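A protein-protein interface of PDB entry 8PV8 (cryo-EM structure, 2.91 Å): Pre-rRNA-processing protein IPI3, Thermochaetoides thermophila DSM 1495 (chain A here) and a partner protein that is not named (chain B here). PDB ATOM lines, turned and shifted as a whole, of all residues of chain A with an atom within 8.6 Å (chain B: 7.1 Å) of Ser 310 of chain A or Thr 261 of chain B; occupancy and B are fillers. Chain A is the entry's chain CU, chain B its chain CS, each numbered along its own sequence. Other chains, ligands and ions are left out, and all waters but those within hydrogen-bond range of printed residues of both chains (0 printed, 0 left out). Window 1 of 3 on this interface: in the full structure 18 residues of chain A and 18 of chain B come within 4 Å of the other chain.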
ATOM      1  N   PHE A 273     -31.535   6.061 -31.753  1.00  0.00           N
ATOM      2  CA  PHE A 273     -30.649   7.172 -31.424  1.00  0.00           C
ATOM      3  C   PHE A 273     -29.386   7.123 -32.275  1.00  0.00           C
ATOM      4  O   PHE A 273     -28.972   8.140 -32.844  1.00  0.00           O
ATOM      5  CB  PHE A 273     -30.303   7.147 -29.934  1.00  0.00           C
ATOM      6  CG  PHE A 273     -29.239   8.136 -29.534  1.00  0.00           C
ATOM      7  CD1 PHE A 273     -29.323   9.468 -29.915  1.00  0.00           C
ATOM      8  CD2 PHE A 273     -28.151   7.728 -28.781  1.00  0.00           C
ATOM      9  CE1 PHE A 273     -28.344  10.372 -29.548  1.00  0.00           C
ATOM     10  CE2 PHE A 273     -27.168   8.628 -28.412  1.00  0.00           C
ATOM     11  CZ  PHE A 273     -27.265   9.951 -28.795  1.00  0.00           C
ATOM     12  N   GLY A 292     -22.579  11.564 -17.362  1.00  0.00           N
ATOM     13  CA  GLY A 292     -23.666  10.957 -18.096  1.00  0.00           C
ATOM     14  C   GLY A 292     -23.879  11.510 -19.486  1.00  0.00           C
ATOM     15  O   GLY A 292     -24.784  11.045 -20.188  1.00  0.00           O
ATOM     16  N   THR A 293     -23.077  12.489 -19.903  1.00  0.00           N
ATOM     17  CA  THR A 293     -23.274  13.093 -21.214  1.00  0.00           C
ATOM     18  C   THR A 293     -22.670  12.233 -22.316  1.00  0.00           C
ATOM     19  O   THR A 293     -23.018  12.386 -23.492  1.00  0.00           O
ATOM     20  CB  THR A 293     -22.666  14.492 -21.238  1.00  0.00           C
ATOM     21  OG1 THR A 293     -21.246  14.395 -21.076  1.00  0.00           O
ATOM     22  CG2 THR A 293     -23.233  15.327 -20.108  1.00  0.00           C
ATOM     23  N   MET A 294     -21.763  11.327 -21.960  1.00  0.00           N
ATOM     24  CA  MET A 294     -21.005  10.562 -22.938  1.00  0.00           C
ATOM     25  C   MET A 294     -21.075   9.071 -22.639  1.00  0.00           C
ATOM     26  O   MET A 294     -21.212   8.658 -21.483  1.00  0.00           O
ATOM     27  CB  MET A 294     -19.546  11.034 -22.989  1.00  0.00           C
ATOM     28  CG  MET A 294     -19.405  12.509 -23.371  1.00  0.00           C
ATOM     29  SD  MET A 294     -17.927  13.334 -22.759  1.00  0.00           S
ATOM     30  CE  MET A 294     -16.765  11.983 -22.791  1.00  0.00           C
ATOM     31  N   LEU A 295     -21.000   8.272 -23.702  1.00  0.00           N
ATOM     32  CA  LEU A 295     -21.094   6.820 -23.633  1.00  0.00           C
ATOM     33  C   LEU A 295     -19.899   6.203 -24.342  1.00  0.00           C
ATOM     34  O   LEU A 295     -19.370   6.785 -25.294  1.00  0.00           O
ATOM     35  CB  LEU A 295     -22.387   6.313 -24.275  1.00  0.00           C
ATOM     36  CG  LEU A 295     -23.629   6.078 -23.417  1.00  0.00           C
ATOM     37  CD1 LEU A 295     -24.132   7.361 -22.795  1.00  0.00           C
ATOM     38  CD2 LEU A 295     -24.712   5.445 -24.269  1.00  0.00           C
ATOM     39  N   TRP A 307     -19.864   8.115 -27.763  1.00  0.00           N
ATOM     40  CA  TRP A 307     -21.134   8.716 -28.143  1.00  0.00           C
ATOM     41  C   TRP A 307     -21.393   9.920 -27.250  1.00  0.00           C
ATOM     42  O   TRP A 307     -21.475   9.777 -26.028  1.00  0.00           O
ATOM     43  CB  TRP A 307     -22.291   7.723 -28.004  1.00  0.00           C
ATOM     44  CG  TRP A 307     -22.095   6.387 -28.661  1.00  0.00           C
ATOM     45  CD1 TRP A 307     -21.229   5.402 -28.284  1.00  0.00           C
ATOM     46  CD2 TRP A 307     -22.819   5.871 -29.784  1.00  0.00           C
ATOM     47  NE1 TRP A 307     -21.350   4.320 -29.116  1.00  0.00           N
ATOM     48  CE2 TRP A 307     -22.321   4.580 -30.044  1.00  0.00           C
ATOM     49  CE3 TRP A 307     -23.831   6.381 -30.603  1.00  0.00           C
ATOM     50  CZ2 TRP A 307     -22.802   3.790 -31.085  1.00  0.00           C
ATOM     51  CZ3 TRP A 307     -24.306   5.594 -31.637  1.00  0.00           C
ATOM     52  CH2 TRP A 307     -23.792   4.313 -31.868  1.00  0.00           C
ATOM     53  N   ASP A 308     -21.531  11.094 -27.855  1.00  0.00           N
ATOM     54  CA  ASP A 308     -21.925  12.300 -27.139  1.00  0.00           C
ATOM     55  C   ASP A 308     -23.402  12.551 -27.409  1.00  0.00           C
ATOM     56  O   ASP A 308     -23.778  12.879 -28.537  1.00  0.00           O
ATOM     57  CB  ASP A 308     -21.082  13.502 -27.567  1.00  0.00           C
ATOM     58  CG  ASP A 308     -19.602  13.295 -27.318  1.00  0.00           C
ATOM     59  OD1 ASP A 308     -19.231  12.219 -26.806  1.00  0.00           O
ATOM     60  OD2 ASP A 308     -18.811  14.212 -27.623  1.00  0.00           O
ATOM     61  N   ILE A 309     -24.230  12.395 -26.370  1.00  0.00           N
ATOM     62  CA  ILE A 309     -25.683  12.408 -26.545  1.00  0.00           C
ATOM     63  C   ILE A 309     -26.167  13.775 -27.013  1.00  0.00           C
ATOM     64  O   ILE A 309     -27.002  13.876 -27.921  1.00  0.00           O
ATOM     65  CB  ILE A 309     -26.381  11.986 -25.240  1.00  0.00           C
ATOM     66  CG1 ILE A 309     -25.699  10.760 -24.637  1.00  0.00           C
ATOM     67  CG2 ILE A 309     -27.852  11.706 -25.491  1.00  0.00           C
ATOM     68  CD1 ILE A 309     -26.190  10.423 -23.248  1.00  0.00           C
ATOM     69  N   SER A 310     -25.657  14.843 -26.406  1.00  0.00           N
ATOM     70  CA  SER A 310     -26.088  16.189 -26.759  1.00  0.00           C
ATOM     71  C   SER A 310     -25.520  16.634 -28.102  1.00  0.00           C
ATOM     72  O   SER A 310     -26.227  17.249 -28.906  1.00  0.00           O
ATOM     73  CB  SER A 310     -25.684  17.178 -25.665  1.00  0.00           C
ATOM     74  N   GLU A 311     -24.247  16.322 -28.358  1.00  0.00           N
ATOM     75  CA  GLU A 311     -23.559  16.924 -29.496  1.00  0.00           C
ATOM     76  C   GLU A 311     -23.642  16.050 -30.744  1.00  0.00           C
ATOM     77  O   GLU A 311     -24.179  16.477 -31.772  1.00  0.00           O
ATOM     78  CB  GLU A 311     -22.100  17.202 -29.135  1.00  0.00           C
ATOM     79  N   ASN A 312     -23.126  14.824 -30.675  1.00  0.00           N
ATOM     80  CA  ASN A 312     -22.846  14.035 -31.868  1.00  0.00           C
ATOM     81  C   ASN A 312     -23.739  12.806 -31.934  1.00  0.00           C
ATOM     82  O   ASN A 312     -23.591  11.880 -31.130  1.00  0.00           O
ATOM     83  CB  ASN A 312     -21.373  13.613 -31.898  1.00  0.00           C
ATOM     84  N   LYS A 313     -24.649  12.786 -32.911  1.00  0.00           N
ATOM     85  CA  LYS A 313     -25.431  11.580 -33.162  1.00  0.00           C
ATOM     86  C   LYS A 313     -24.544  10.444 -33.659  1.00  0.00           C
ATOM     87  O   LYS A 313     -24.743   9.283 -33.285  1.00  0.00           O
ATOM     88  CB  LYS A 313     -26.545  11.872 -34.168  1.00  0.00           C
ATOM     89  N   GLN B 130     -28.375  22.535 -37.816  1.00  0.00           N
ATOM     90  CA  GLN B 130     -28.580  21.987 -36.478  1.00  0.00           C
ATOM     91  C   GLN B 130     -27.464  21.024 -36.099  1.00  0.00           C
ATOM     92  O   GLN B 130     -27.167  20.838 -34.913  1.00  0.00           O
ATOM     93  CB  GLN B 130     -29.941  21.292 -36.395  1.00  0.00           C
ATOM     94  CG  GLN B 130     -31.122  22.182 -36.745  1.00  0.00           C
ATOM     95  CD  GLN B 130     -31.048  23.545 -36.082  1.00  0.00           C
ATOM     96  OE1 GLN B 130     -30.947  23.651 -34.859  1.00  0.00           O
ATOM     97  NE2 GLN B 130     -31.096  24.597 -36.890  1.00  0.00           N
ATOM     98  N   PRO B 134     -23.589  22.271 -32.567  1.00  0.00           N
ATOM     99  CA  PRO B 134     -22.875  21.838 -31.350  1.00  0.00           C
ATOM    100  C   PRO B 134     -21.352  21.894 -31.435  1.00  0.00           C
ATOM    101  O   PRO B 134     -20.700  21.847 -30.386  1.00  0.00           O
ATOM    102  CB  PRO B 134     -23.354  20.393 -31.150  1.00  0.00           C
ATOM    103  CG  PRO B 134     -24.623  20.308 -31.888  1.00  0.00           C
ATOM    104  CD  PRO B 134     -24.399  21.154 -33.094  1.00  0.00           C
ATOM    105  N   HIS B 135     -20.762  21.995 -32.625  1.00  0.00           N
ATOM    106  CA  HIS B 135     -19.314  21.894 -32.782  1.00  0.00           C
ATOM    107  C   HIS B 135     -18.678  23.226 -33.168  1.00  0.00           C
ATOM    108  O   HIS B 135     -17.767  23.263 -33.993  1.00  0.00           O
ATOM    109  CB  HIS B 135     -18.961  20.822 -33.812  1.00  0.00           C
ATOM    110  CG  HIS B 135     -19.767  19.568 -33.682  1.00  0.00           C
ATOM    111  ND1 HIS B 135     -19.455  18.574 -32.781  1.00  0.00           N
ATOM    112  CD2 HIS B 135     -20.873  19.147 -34.338  1.00  0.00           C
ATOM    113  CE1 HIS B 135     -20.333  17.594 -32.887  1.00  0.00           C
ATOM    114  NE2 HIS B 135     -21.205  17.917 -33.826  1.00  0.00           N
ATOM    115  N   LEU B 258     -33.026  14.245 -19.427  1.00  0.00           N
ATOM    116  CA  LEU B 258     -31.648  14.473 -19.825  1.00  0.00           C
ATOM    117  C   LEU B 258     -31.480  15.884 -20.392  1.00  0.00           C
ATOM    118  O   LEU B 258     -32.423  16.449 -20.953  1.00  0.00           O
ATOM    119  CB  LEU B 258     -31.222  13.440 -20.864  1.00  0.00           C
ATOM    120  CG  LEU B 258     -31.141  11.993 -20.381  1.00  0.00           C
ATOM    121  CD1 LEU B 258     -30.834  11.071 -21.545  1.00  0.00           C
ATOM    122  CD2 LEU B 258     -30.097  11.851 -19.291  1.00  0.00           C
ATOM    123  N   PRO B 259     -30.297  16.478 -20.239  1.00  0.00           N
ATOM    124  CA  PRO B 259     -30.073  17.824 -20.784  1.00  0.00           C
ATOM    125  C   PRO B 259     -30.073  17.819 -22.307  1.00  0.00           C
ATOM    126  O   PRO B 259     -29.365  17.035 -22.943  1.00  0.00           O
ATOM    127  CB  PRO B 259     -28.700  18.208 -20.221  1.00  0.00           C
ATOM    128  CG  PRO B 259     -28.521  17.331 -19.024  1.00  0.00           C
ATOM    129  CD  PRO B 259     -29.171  16.040 -19.397  1.00  0.00           C
ATOM    130  N   THR B 260     -30.879  18.705 -22.887  1.00  0.00           N
ATOM    131  CA  THR B 260     -30.983  18.843 -24.333  1.00  0.00           C
ATOM    132  C   THR B 260     -30.061  19.917 -24.894  1.00  0.00           C
ATOM    133  O   THR B 260     -30.004  20.088 -26.115  1.00  0.00           O
ATOM    134  CB  THR B 260     -32.428  19.152 -24.732  1.00  0.00           C
ATOM    135  OG1 THR B 260     -32.805  20.434 -24.215  1.00  0.00           O
ATOM    136  CG2 THR B 260     -33.370  18.093 -24.181  1.00  0.00           C
ATOM    137  N   THR B 261     -29.346  20.639 -24.039  1.00  0.00           N
ATOM    138  CA  THR B 261     -28.410  21.671 -24.467  1.00  0.00           C
ATOM    139  C   THR B 261     -27.149  21.031 -25.042  1.00  0.00           C
ATOM    140  O   THR B 261     -26.562  20.147 -24.411  1.00  0.00           O
ATOM    141  CB  THR B 261     -28.033  22.575 -23.296  1.00  0.00           C
ATOM    142  OG1 THR B 261     -29.222  23.104 -22.697  1.00  0.00           O
ATOM    143  CG2 THR B 261     -27.155  23.727 -23.763  1.00  0.00           C
ATOM    144  N   PRO B 262     -26.737  21.435 -26.245  1.00  0.00           N
ATOM    145  CA  PRO B 262     -25.465  20.948 -26.787  1.00  0.00           C
ATOM    146  C   PRO B 262     -24.288  21.405 -25.941  1.00  0.00           C
ATOM    147  O   PRO B 262     -24.196  22.568 -25.541  1.00  0.00           O
ATOM    148  CB  PRO B 262     -25.416  21.564 -28.190  1.00  0.00           C
ATOM    149  CG  PRO B 262     -26.346  22.734 -28.127  1.00  0.00           C
ATOM    150  CD  PRO B 262     -27.437  22.320 -27.190  1.00  0.00           C
ATOM    151  N   ASN B 263     -23.374  20.462 -25.700  1.00  0.00           N
ATOM    152  CA  ASN B 263     -22.288  20.606 -24.736  1.00  0.00           C
ATOM    153  C   ASN B 263     -22.767  21.102 -23.367  1.00  0.00           C
ATOM    154  O   ASN B 263     -22.504  22.246 -22.989  1.00  0.00           O
ATOM    155  CB  ASN B 263     -21.192  21.518 -25.272  1.00  0.00           C
ATOM    156  CG  ASN B 263     -20.468  20.923 -26.459  1.00  0.00           C
ATOM    157  OD1 ASN B 263     -20.513  21.465 -27.560  1.00  0.00           O
ATOM    158  ND2 ASN B 263     -19.791  19.803 -26.237  1.00  0.00           N
ATOM    159  N   PRO B 264     -23.476  20.270 -22.607  1.00  0.00           N
ATOM    160  CA  PRO B 264     -23.867  20.676 -21.256  1.00  0.00           C
ATOM    161  C   PRO B 264     -22.682  20.606 -20.308  1.00  0.00           C
ATOM    162  O   PRO B 264     -21.668  19.961 -20.583  1.00  0.00           O
ATOM    163  CB  PRO B 264     -24.945  19.658 -20.881  1.00  0.00           C
ATOM    164  CG  PRO B 264     -24.540  18.433 -21.609  1.00  0.00           C
ATOM    165  CD  PRO B 264     -23.867  18.876 -22.888  1.00  0.00           C
ATOM    166  N   PHE B 265     -22.825  21.314 -19.184  1.00  0.00           N
ATOM    167  CA  PHE B 265     -21.818  21.436 -18.130  1.00  0.00           C
ATOM    168  C   PHE B 265     -20.503  22.017 -18.632  1.00  0.00           C
ATOM    169  O   PHE B 265     -19.445  21.742 -18.059  1.00  0.00           O
ATOM    170  CB  PHE B 265     -21.560  20.095 -17.432  1.00  0.00           C
ATOM    171  CG  PHE B 265     -22.810  19.382 -17.020  1.00  0.00           C
ATOM    172  CD1 PHE B 265     -23.641  19.918 -16.053  1.00  0.00           C
ATOM    173  CD2 PHE B 265     -23.154  18.172 -17.599  1.00  0.00           C
ATOM    174  CE1 PHE B 265     -24.792  19.265 -15.675  1.00  0.00           C
ATOM    175  CE2 PHE B 265     -24.305  17.513 -17.221  1.00  0.00           C
ATOM    176  CZ  PHE B 265     -25.126  18.061 -16.258  1.00  0.00           C
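The backbone NH (N) of Ile 309 of chain A is in hydrogen-bond range of the backbone carbonyl oxygen (O) of Thr 293 of chain A, at 3.1 Å.
The backbone carbonyl oxygen (O) of Pro 134 of chain B sits close to the side-chain amide oxygen (OD1) of Asn 263 of chain B (2.9 Å).
Among the printed residues, pairs that only touch across the chains: Thr 293 of chain A with Pro 264 of chain B (3.7 Å), Thr 293 of chain A with Phe 265 of chain B (3.8 Å), Ser 310 of chain A with Thr 261 of chain B (3.3 Å), Ser 310 of chain A with Pro 262 of chain B (3.9 Å), Ser 310 of chain A with Pro 264 of chain B (3.7 Å), Glu 311 of chain A with Pro 134 of chain B (3.8 Å) and Glu 311 of chain A with His 135 of chain B (3.9 Å).
Of the printed residues of chain B, Ser 310 of chain A touches Thr 261, Pro 262 and Pro 264.
Printed residues of chain B within 4 Å of Glu 311 of chain A: Pro 134 and His 135.
Gln 130 of chain B touches none of the printed residues of chain A.
Of the printed residues of chain A, Pro 262 of chain B touches Ser 310 (3.9 Å).
Of the printed residues of chain A, Pro 264 of chain B touches Thr 293 (3.7 Å) and Ser 310 (3.7 Å).
The nearest residue of chain A that does not touch Thr 261 of chain B is Glu 311 of chain A (6.0 Å).
Of the 12 printed residues of chain A, 3 touch a printed residue of chain B.
Printed residues of chain A that touch a printed residue of chain B: Thr 293, Ser 310 and Glu 311.
Hydrophobic or aromatic side chains of chain B within 4 Å of the printed part of chain A: Pro 134, His 135, Pro 264 and Phe 265.
Among the printed residues, 7 pairs touch across the chains.
Among the printed residues, no Asp or Glu carboxylate lies within 4 Å of a Lys or Arg side-chain nitrogen of the other chain.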
